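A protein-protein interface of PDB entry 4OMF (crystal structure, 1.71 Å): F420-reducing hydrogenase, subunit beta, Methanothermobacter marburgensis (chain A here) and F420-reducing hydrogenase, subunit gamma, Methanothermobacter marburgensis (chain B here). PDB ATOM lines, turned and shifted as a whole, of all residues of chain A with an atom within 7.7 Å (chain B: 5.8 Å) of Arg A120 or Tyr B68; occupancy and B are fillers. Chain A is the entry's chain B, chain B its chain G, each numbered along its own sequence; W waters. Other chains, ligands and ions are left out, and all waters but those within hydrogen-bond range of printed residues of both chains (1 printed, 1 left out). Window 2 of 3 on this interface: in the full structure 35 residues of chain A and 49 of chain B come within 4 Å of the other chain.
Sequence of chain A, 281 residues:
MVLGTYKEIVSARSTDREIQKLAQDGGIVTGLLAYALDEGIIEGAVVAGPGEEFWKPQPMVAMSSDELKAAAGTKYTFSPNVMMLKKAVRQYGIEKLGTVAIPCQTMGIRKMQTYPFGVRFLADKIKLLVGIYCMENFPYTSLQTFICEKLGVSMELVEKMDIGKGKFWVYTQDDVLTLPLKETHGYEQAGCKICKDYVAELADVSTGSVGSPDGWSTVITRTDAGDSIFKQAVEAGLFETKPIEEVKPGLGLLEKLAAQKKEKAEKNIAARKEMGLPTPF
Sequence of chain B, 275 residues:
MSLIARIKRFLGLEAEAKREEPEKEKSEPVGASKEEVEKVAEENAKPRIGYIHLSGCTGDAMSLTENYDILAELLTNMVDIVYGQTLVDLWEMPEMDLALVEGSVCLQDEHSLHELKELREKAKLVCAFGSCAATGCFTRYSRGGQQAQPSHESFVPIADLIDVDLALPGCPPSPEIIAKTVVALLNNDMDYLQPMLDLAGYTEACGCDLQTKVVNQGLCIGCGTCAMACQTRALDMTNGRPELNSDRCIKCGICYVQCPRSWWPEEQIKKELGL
The backbone carbonyl oxygen (O) of Phe A117 sits at hydrogen-bond distance from the backbone NH (N) of Ser B174 (3.0 Å). The backbone NH of Phe A121 is in hydrogen-bond range of the side-chain carboxylate of Glu B176, 3.0 Å away. O of Gly A118 lies close to NE2 of Gln B231 (3.4 Å). OE1 of Glu B66 lies within salt-bridge range of NH2 of Arg A120 (2.9 Å). The backbone carbonyl oxygen (O) of Pro A116 sits at hydrogen-bond distance from the side-chain hydroxyl (OG) of Ser B174 (2.7 Å).
The backbone carbonyl oxygen (O) of Phe A121 is in hydrogen-bond range of the side-chain amino group (NZ) of Lys A125, at 2.9 Å. NH2 of Arg A90 lies within hydrogen-bond range of O of Arg A120, 2.9 Å away. ND2 of Asn B67 lies within hydrogen-bond range of O of Pro B175. The side-chain hydroxyl of Ser B174 lies close to the backbone NH of Glu B176. OE1 of Glu B66 is in hydrogen-bond range of OH of Tyr B68 (2.5 Å).
Among the printed residues, merely in contact across the chains: Val A119 with Ser B174, Phe A121 with Tyr B68, Phe A121 with Glu B66, Phe A121 with Pro B175, Arg A120 with Tyr B68, Arg A120 with Ser B174, Pro A116 with Glu B176, Arg A120 with Glu B176, Arg A120 with Pro B175 and Leu A122 with Glu B176.
Arg A120 touches just these residues of chain B: Glu B66 (2.9 Å), Tyr B68 (3.8 Å), Ser B174 (3.9 Å), Pro B175 (3.9 Å) and Glu B176 (3.9 Å). Tyr B68 touches just these residues of chain A: Arg A120 (3.8 Å) and Phe A121 (3.5 Å). Printed residues of chain B within 4 Å of Gly A118: Gln B231. Of the printed residues of chain B, Phe A121 touches Glu B66 (3.8 Å), Tyr B68 (3.5 Å), Pro B175 (3.8 Å) and Glu B176 (3.0 Å). Lys A125 touches none of the printed residues of chain B. Asp B69 touches none of the printed residues of chain A. The nearest residue of chain B that does not touch Arg A120 is Ser B63 (5.0 Å). The nearest printed residue of chain A that does not touch Tyr B68 is Lys A125 (9.2 Å).
Hydrophobic or aromatic side chains of chain A within 4 Å of the printed part of chain B: Pro A116 and Phe A121. Of the 13 printed residues of chain B, 6 touch a printed residue of chain A. Among the printed residues, 15 pairs touch across the chains.
Water W1 lies within hydrogen-bond range of OG of Ser B63 (2.8 Å) and NH1 of Arg A120 (2.8 Å).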
ATOM      1  N   LYS A  86       4.757  22.651 -25.511  1.00  0.00           N
ATOM      2  CA  LYS A  86       4.706  21.600 -24.486  1.00  0.00           C
ATOM      3  C   LYS A  86       3.590  20.590 -24.770  1.00  0.00           C
ATOM      4  O   LYS A  86       3.821  19.399 -24.589  1.00  0.00           O
ATOM      5  CB  LYS A  86       4.550  22.132 -23.059  1.00  0.00           C
ATOM      6  CG  LYS A  86       4.799  20.972 -22.018  1.00  0.00           C
ATOM      7  CD  LYS A  86       4.278  21.283 -20.641  1.00  0.00           C
ATOM      8  CE  LYS A  86       5.084  22.394 -20.014  1.00  0.00           C
ATOM      9  NZ  LYS A  86       4.353  22.982 -18.851  1.00  0.00           N
ATOM     10  N   VAL A  89       4.827  17.775 -26.898  1.00  0.00           N
ATOM     11  CA  VAL A  89       5.654  16.690 -26.358  1.00  0.00           C
ATOM     12  C   VAL A  89       4.917  15.912 -25.255  1.00  0.00           C
ATOM     13  O   VAL A  89       5.443  14.921 -24.727  1.00  0.00           O
ATOM     14  CB  VAL A  89       7.002  17.211 -25.833  1.00  0.00           C
ATOM     15  CG1 VAL A  89       7.822  17.863 -26.983  1.00  0.00           C
ATOM     16  CG2 VAL A  89       6.811  18.189 -24.664  1.00  0.00           C
ATOM     17  N   ARG A  90       3.703  16.338 -24.911  1.00  0.00           N
ATOM     18  CA  ARG A  90       2.900  15.559 -23.967  1.00  0.00           C
ATOM     19  C   ARG A  90       1.929  14.672 -24.738  1.00  0.00           C
ATOM     20  O   ARG A  90       2.337  13.625 -25.228  1.00  0.00           O
ATOM     21  CB  ARG A  90       2.198  16.473 -22.968  1.00  0.00           C
ATOM     22  CG  ARG A  90       3.209  17.339 -22.173  1.00  0.00           C
ATOM     23  CD  ARG A  90       4.078  16.525 -21.213  1.00  0.00           C
ATOM     24  NE  ARG A  90       4.610  17.410 -20.176  1.00  0.00           N
ATOM     25  CZ  ARG A  90       5.884  17.790 -20.088  1.00  0.00           C
ATOM     26  NH1 ARG A  90       6.792  17.337 -20.946  1.00  0.00           N
ATOM     27  NH2 ARG A  90       6.250  18.608 -19.116  1.00  0.00           N
ATOM     28  N   MET A 112      14.033  29.292 -22.707  1.00  0.00           N
ATOM     29  CA  MET A 112      13.515  28.109 -22.038  1.00  0.00           C
ATOM     30  C   MET A 112      14.553  26.995 -22.046  1.00  0.00           C
ATOM     31  O   MET A 112      14.739  26.314 -21.032  1.00  0.00           O
ATOM     32  CB  MET A 112      12.209  27.625 -22.701  1.00  0.00           C
ATOM     33  CG  MET A 112      11.726  26.250 -22.216  1.00  0.00           C
ATOM     34  SD  MET A 112      12.362  24.857 -23.202  1.00  0.00           S
ATOM     35  CE  MET A 112      11.629  25.219 -24.823  1.00  0.00           C
ATOM     36  N   PRO A 116      15.316  26.222 -18.106  1.00  0.00           N
ATOM     37  CA  PRO A 116      13.980  25.607 -18.079  1.00  0.00           C
ATOM     38  C   PRO A 116      13.419  25.486 -16.664  1.00  0.00           C
ATOM     39  O   PRO A 116      13.084  24.373 -16.257  1.00  0.00           O
ATOM     40  CB  PRO A 116      14.230  24.227 -18.682  1.00  0.00           C
ATOM     41  CG  PRO A 116      15.668  23.909 -18.249  1.00  0.00           C
ATOM     42  CD  PRO A 116      16.378  25.238 -18.419  1.00  0.00           C
ATOM     43  N   PHE A 117      13.317  26.599 -15.943  1.00  0.00           N
ATOM     44  CA  PHE A 117      12.877  26.559 -14.552  1.00  0.00           C
ATOM     45  C   PHE A 117      11.606  25.745 -14.377  1.00  0.00           C
ATOM     46  O   PHE A 117      11.606  24.789 -13.602  1.00  0.00           O
ATOM     47  CB  PHE A 117      12.642  27.961 -14.000  1.00  0.00           C
ATOM     48  CG  PHE A 117      13.893  28.684 -13.671  1.00  0.00           C
ATOM     49  CD1 PHE A 117      14.516  29.499 -14.621  1.00  0.00           C
ATOM     50  CD2 PHE A 117      14.460  28.557 -12.407  1.00  0.00           C
ATOM     51  CE1 PHE A 117      15.685  30.172 -14.296  1.00  0.00           C
ATOM     52  CE2 PHE A 117      15.619  29.219 -12.090  1.00  0.00           C
ATOM     53  CZ  PHE A 117      16.228  30.027 -13.028  1.00  0.00           C
ATOM     54  N   GLY A 118      10.556  26.087 -15.121  1.00  0.00           N
ATOM     55  CA  GLY A 118       9.276  25.400 -14.933  1.00  0.00           C
ATOM     56  C   GLY A 118       8.922  24.439 -16.066  1.00  0.00           C
ATOM     57  O   GLY A 118       7.769  24.031 -16.203  1.00  0.00           O
ATOM     58  N   VAL A 119       9.903  24.095 -16.893  1.00  0.00           N
ATOM     59  CA  VAL A 119       9.608  23.371 -18.145  1.00  0.00           C
ATOM     60  C   VAL A 119      10.334  22.021 -18.165  1.00  0.00           C
ATOM     61  O   VAL A 119      11.546  21.940 -18.396  1.00  0.00           O
ATOM     62  CB  VAL A 119       9.987  24.221 -19.382  1.00  0.00           C
ATOM     63  CG1 VAL A 119       9.537  23.540 -20.671  1.00  0.00           C
ATOM     64  CG2 VAL A 119       9.327  25.614 -19.282  1.00  0.00           C
ATOM     65  N   ARG A 120       9.575  20.978 -17.854  1.00  0.00           N
ATOM     66  CA  ARG A 120      10.078  19.615 -17.705  1.00  0.00           C
ATOM     67  C   ARG A 120      10.102  18.858 -19.035  1.00  0.00           C
ATOM     68  O   ARG A 120       9.088  18.791 -19.685  1.00  0.00           O
ATOM     69  CB  ARG A 120       9.179  18.874 -16.694  1.00  0.00           C
ATOM     70  CG  ARG A 120       9.373  17.370 -16.553  1.00  0.00           C
ATOM     71  CD  ARG A 120       8.237  16.834 -15.652  1.00  0.00           C
ATOM     72  NE  ARG A 120       8.130  15.371 -15.728  1.00  0.00           N
ATOM     73  CZ  ARG A 120       8.534  14.519 -14.789  1.00  0.00           C
ATOM     74  NH1 ARG A 120       9.051  14.953 -13.643  1.00  0.00           N
ATOM     75  NH2 ARG A 120       8.391  13.213 -14.994  1.00  0.00           N
ATOM     76  N   PHE A 121      11.259  18.302 -19.413  1.00  0.00           N
ATOM     77  CA  PHE A 121      11.401  17.408 -20.574  1.00  0.00           C
ATOM     78  C   PHE A 121      10.799  17.978 -21.868  1.00  0.00           C
ATOM     79  O   PHE A 121       9.979  17.326 -22.547  1.00  0.00           O
ATOM     80  CB  PHE A 121      10.773  16.041 -20.267  1.00  0.00           C
ATOM     81  CG  PHE A 121      11.373  15.340 -19.059  1.00  0.00           C
ATOM     82  CD1 PHE A 121      12.678  15.594 -18.660  1.00  0.00           C
ATOM     83  CD2 PHE A 121      10.629  14.427 -18.333  1.00  0.00           C
ATOM     84  CE1 PHE A 121      13.235  14.943 -17.553  1.00  0.00           C
ATOM     85  CE2 PHE A 121      11.191  13.765 -17.219  1.00  0.00           C
ATOM     86  CZ  PHE A 121      12.493  14.033 -16.842  1.00  0.00           C
ATOM     87  N   LEU A 122      11.209  19.198 -22.195  1.00  0.00           N
ATOM     88  CA  LEU A 122      10.909  19.792 -23.494  1.00  0.00           C
ATOM     89  C   LEU A 122      12.179  20.250 -24.204  1.00  0.00           C
ATOM     90  O   LEU A 122      12.338  20.010 -25.396  1.00  0.00           O
ATOM     91  CB  LEU A 122       9.934  20.961 -23.345  1.00  0.00           C
ATOM     92  CG  LEU A 122       9.815  21.835 -24.607  1.00  0.00           C
ATOM     93  CD1 LEU A 122       9.301  20.990 -25.800  1.00  0.00           C
ATOM     94  CD2 LEU A 122       8.884  22.976 -24.342  1.00  0.00           C
ATOM     95  N   ALA A 123      13.100  20.869 -23.461  1.00  0.00           N
ATOM     96  CA  ALA A 123      14.225  21.585 -24.079  1.00  0.00           C
ATOM     97  C   ALA A 123      15.022  20.744 -25.083  1.00  0.00           C
ATOM     98  O   ALA A 123      15.320  21.199 -26.187  1.00  0.00           O
ATOM     99  CB  ALA A 123      15.144  22.111 -23.006  1.00  0.00           C
ATOM    100  N   LYS A 125      14.076  18.194 -26.727  1.00  0.00           N
ATOM    101  CA  LYS A 125      13.252  17.620 -27.793  1.00  0.00           C
ATOM    102  C   LYS A 125      13.135  18.503 -29.020  1.00  0.00           C
ATOM    103  O   LYS A 125      12.680  18.045 -30.066  1.00  0.00           O
ATOM    104  CB  LYS A 125      11.856  17.300 -27.240  1.00  0.00           C
ATOM    105  CG  LYS A 125      11.933  16.102 -26.290  1.00  0.00           C
ATOM    106  CD  LYS A 125      10.668  15.891 -25.498  1.00  0.00           C
ATOM    107  CE  LYS A 125      10.876  14.815 -24.411  1.00  0.00           C
ATOM    108  NZ  LYS A 125       9.611  14.646 -23.629  1.00  0.00           N
ATOM    109  N   SER B  63      11.603  15.678  -8.274  1.00  0.00           N
ATOM    110  CA  SER B  63      12.113  16.201  -9.547  1.00  0.00           C
ATOM    111  C   SER B  63      13.633  16.039  -9.674  1.00  0.00           C
ATOM    112  O   SER B  63      14.131  15.624 -10.716  1.00  0.00           O
ATOM    113  CB  SER B  63      11.742  17.677  -9.713  1.00  0.00           C
ATOM    114  OG  SER B  63      11.962  18.100 -11.066  1.00  0.00           O
ATOM    115  N   THR B  65      15.344  13.806  -8.372  1.00  0.00           N
ATOM    116  CA  THR B  65      15.681  12.397  -8.553  1.00  0.00           C
ATOM    117  C   THR B  65      15.231  11.872  -9.918  1.00  0.00           C
ATOM    118  O   THR B  65      15.548  10.750 -10.269  1.00  0.00           O
ATOM    119  CB  THR B  65      15.064  11.479  -7.456  1.00  0.00           C
ATOM    120  OG1 THR B  65      13.628  11.527  -7.505  1.00  0.00           O
ATOM    121  CG2 THR B  65      15.578  11.852  -6.040  1.00  0.00           C
ATOM    122  N   GLU B  66      14.510  12.678 -10.699  1.00  0.00           N
ATOM    123  CA  GLU B  66      14.135  12.249 -12.035  1.00  0.00           C
ATOM    124  C   GLU B  66      15.187  12.664 -13.079  1.00  0.00           C
ATOM    125  O   GLU B  66      14.929  12.622 -14.275  1.00  0.00           O
ATOM    126  CB  GLU B  66      12.733  12.780 -12.389  1.00  0.00           C
ATOM    127  CG  GLU B  66      11.663  11.994 -11.602  1.00  0.00           C
ATOM    128  CD  GLU B  66      10.258  12.077 -12.246  1.00  0.00           C
ATOM    129  OE1 GLU B  66      10.096  11.592 -13.374  1.00  0.00           O
ATOM    130  OE2 GLU B  66       9.342  12.614 -11.606  1.00  0.00           O
ATOM    131  N   ASN B  67      16.379  13.046 -12.612  1.00  0.00           N
ATOM    132  CA  ASN B  67      17.578  12.995 -13.434  1.00  0.00           C
ATOM    133  C   ASN B  67      18.069  11.558 -13.461  1.00  0.00           C
ATOM    134  O   ASN B  67      19.044  11.217 -12.798  1.00  0.00           O
ATOM    135  CB  ASN B  67      18.637  13.951 -12.883  1.00  0.00           C
ATOM    136  CG  ASN B  67      18.285  15.379 -13.164  1.00  0.00           C
ATOM    137  OD1 ASN B  67      18.311  15.788 -14.318  1.00  0.00           O
ATOM    138  ND2 ASN B  67      17.899  16.139 -12.136  1.00  0.00           N
ATOM    139  N   TYR B  68      17.351  10.713 -14.206  1.00  0.00           N
ATOM    140  CA  TYR B  68      17.457   9.269 -14.030  1.00  0.00           C
ATOM    141  C   TYR B  68      18.853   8.729 -14.282  1.00  0.00           C
ATOM    142  O   TYR B  68      19.394   7.982 -13.468  1.00  0.00           O
ATOM    143  CB  TYR B  68      16.493   8.532 -14.958  1.00  0.00           C
ATOM    144  CG  TYR B  68      15.113   9.127 -15.044  1.00  0.00           C
ATOM    145  CD1 TYR B  68      14.722   9.828 -16.181  1.00  0.00           C
ATOM    146  CD2 TYR B  68      14.183   8.962 -14.007  1.00  0.00           C
ATOM    147  CE1 TYR B  68      13.458  10.369 -16.302  1.00  0.00           C
ATOM    148  CE2 TYR B  68      12.914   9.510 -14.116  1.00  0.00           C
ATOM    149  CZ  TYR B  68      12.563  10.217 -15.273  1.00  0.00           C
ATOM    150  OH  TYR B  68      11.300  10.764 -15.425  1.00  0.00           O
ATOM    151  N   ASP B  69      19.428   9.099 -15.425  1.00  0.00           N
ATOM    152  CA  ASP B  69      20.660   8.472 -15.857  1.00  0.00           C
ATOM    153  C   ASP B  69      21.831   8.810 -14.952  1.00  0.00           C
ATOM    154  O   ASP B  69      22.709   7.961 -14.702  1.00  0.00           O
ATOM    155  CB  ASP B  69      20.998   8.877 -17.288  1.00  0.00           C
ATOM    156  CG  ASP B  69      20.051   8.269 -18.301  1.00  0.00           C
ATOM    157  OD1 ASP B  69      19.179   7.451 -17.908  1.00  0.00           O
ATOM    158  OD2 ASP B  69      20.192   8.608 -19.493  1.00  0.00           O
ATOM    159  N   ILE B  70      21.838  10.030 -14.422  1.00  0.00           N
ATOM    160  CA  ILE B  70      22.993  10.467 -13.645  1.00  0.00           C
ATOM    161  C   ILE B  70      22.831  10.307 -12.141  1.00  0.00           C
ATOM    162  O   ILE B  70      23.791  10.470 -11.402  1.00  0.00           O
ATOM    163  CB  ILE B  70      23.339  11.936 -13.922  1.00  0.00           C
ATOM    164  CG1 ILE B  70      22.288  12.872 -13.324  1.00  0.00           C
ATOM    165  CG2 ILE B  70      23.550  12.153 -15.408  1.00  0.00           C
ATOM    166  CD1 ILE B  70      22.679  14.326 -13.397  1.00  0.00           C
ATOM    167  N   LEU B  71      21.635   9.953 -11.691  1.00  0.00           N
ATOM    168  CA  LEU B  71      21.334   9.999 -10.250  1.00  0.00           C
ATOM    169  C   LEU B  71      22.311   9.211  -9.383  1.00  0.00           C
ATOM    170  O   LEU B  71      22.791   9.727  -8.362  1.00  0.00           O
ATOM    171  CB  LEU B  71      19.904   9.522  -9.983  1.00  0.00           C
ATOM    172  CG  LEU B  71      19.492   9.681  -8.514  1.00  0.00           C
ATOM    173  CD1 LEU B  71      19.489  11.168  -8.138  1.00  0.00           C
ATOM    174  CD2 LEU B  71      18.117   9.017  -8.216  1.00  0.00           C
ATOM    175  N   ALA B  72      22.634   7.983  -9.779  1.00  0.00           N
ATOM    176  CA  ALA B  72      23.530   7.177  -8.959  1.00  0.00           C
ATOM    177  C   ALA B  72      24.897   7.876  -8.835  1.00  0.00           C
ATOM    178  O   ALA B  72      25.430   8.009  -7.736  1.00  0.00           O
ATOM    179  CB  ALA B  72      23.681   5.770  -9.532  1.00  0.00           C
ATOM    180  N   SER B 174      12.109  21.949 -12.979  1.00  0.00           N
ATOM    181  CA  SER B 174      12.356  20.832 -13.865  1.00  0.00           C
ATOM    182  C   SER B 174      13.591  20.031 -13.428  1.00  0.00           C
ATOM    183  O   SER B 174      14.503  20.569 -12.797  1.00  0.00           O
ATOM    184  CB  SER B 174      12.545  21.347 -15.296  1.00  0.00           C
ATOM    185  OG  SER B 174      13.848  21.920 -15.467  1.00  0.00           O
ATOM    186  N   PRO B 175      13.637  18.737 -13.770  1.00  0.00           N
ATOM    187  CA  PRO B 175      14.848  17.978 -13.435  1.00  0.00           C
ATOM    188  C   PRO B 175      16.061  18.644 -14.064  1.00  0.00           C
ATOM    189  O   PRO B 175      17.108  18.693 -13.451  1.00  0.00           O
ATOM    190  CB  PRO B 175      14.583  16.603 -14.039  1.00  0.00           C
ATOM    191  CG  PRO B 175      13.019  16.486 -13.958  1.00  0.00           C
ATOM    192  CD  PRO B 175      12.588  17.888 -14.361  1.00  0.00           C
ATOM    193  N   GLU B 176      15.878  19.211 -15.256  1.00  0.00           N
ATOM    194  CA  GLU B 176      16.979  19.855 -15.969  1.00  0.00           C
ATOM    195  C   GLU B 176      17.515  21.103 -15.242  1.00  0.00           C
ATOM    196  O   GLU B 176      18.721  21.252 -15.105  1.00  0.00           O
ATOM    197  CB  GLU B 176      16.533  20.220 -17.390  1.00  0.00           C
ATOM    198  CG  GLU B 176      16.157  18.999 -18.260  1.00  0.00           C
ATOM    199  CD  GLU B 176      14.642  18.867 -18.503  1.00  0.00           C
ATOM    200  OE1 GLU B 176      14.209  18.891 -19.680  1.00  0.00           O
ATOM    201  OE2 GLU B 176      13.894  18.733 -17.523  1.00  0.00           O
ATOM    202  N   GLN B 231       2.675  25.397 -15.489  1.00  0.00           N
ATOM    203  CA  GLN B 231       2.572  23.981 -15.194  1.00  0.00           C
ATOM    204  C   GLN B 231       1.151  23.546 -14.825  1.00  0.00           C
ATOM    205  O   GLN B 231       0.876  22.363 -14.809  1.00  0.00           O
ATOM    206  CB  GLN B 231       3.567  23.606 -14.074  1.00  0.00           C
ATOM    207  CG  GLN B 231       5.008  23.657 -14.558  1.00  0.00           C
ATOM    208  CD  GLN B 231       6.030  23.714 -13.422  1.00  0.00           C
ATOM    209  OE1 GLN B 231       6.133  24.727 -12.725  1.00  0.00           O
ATOM    210  NE2 GLN B 231       6.800  22.620 -13.240  1.00  0.00           N
HETATM  211  O   HOH W   1       9.726  17.431 -12.576  1.00  0.00           O
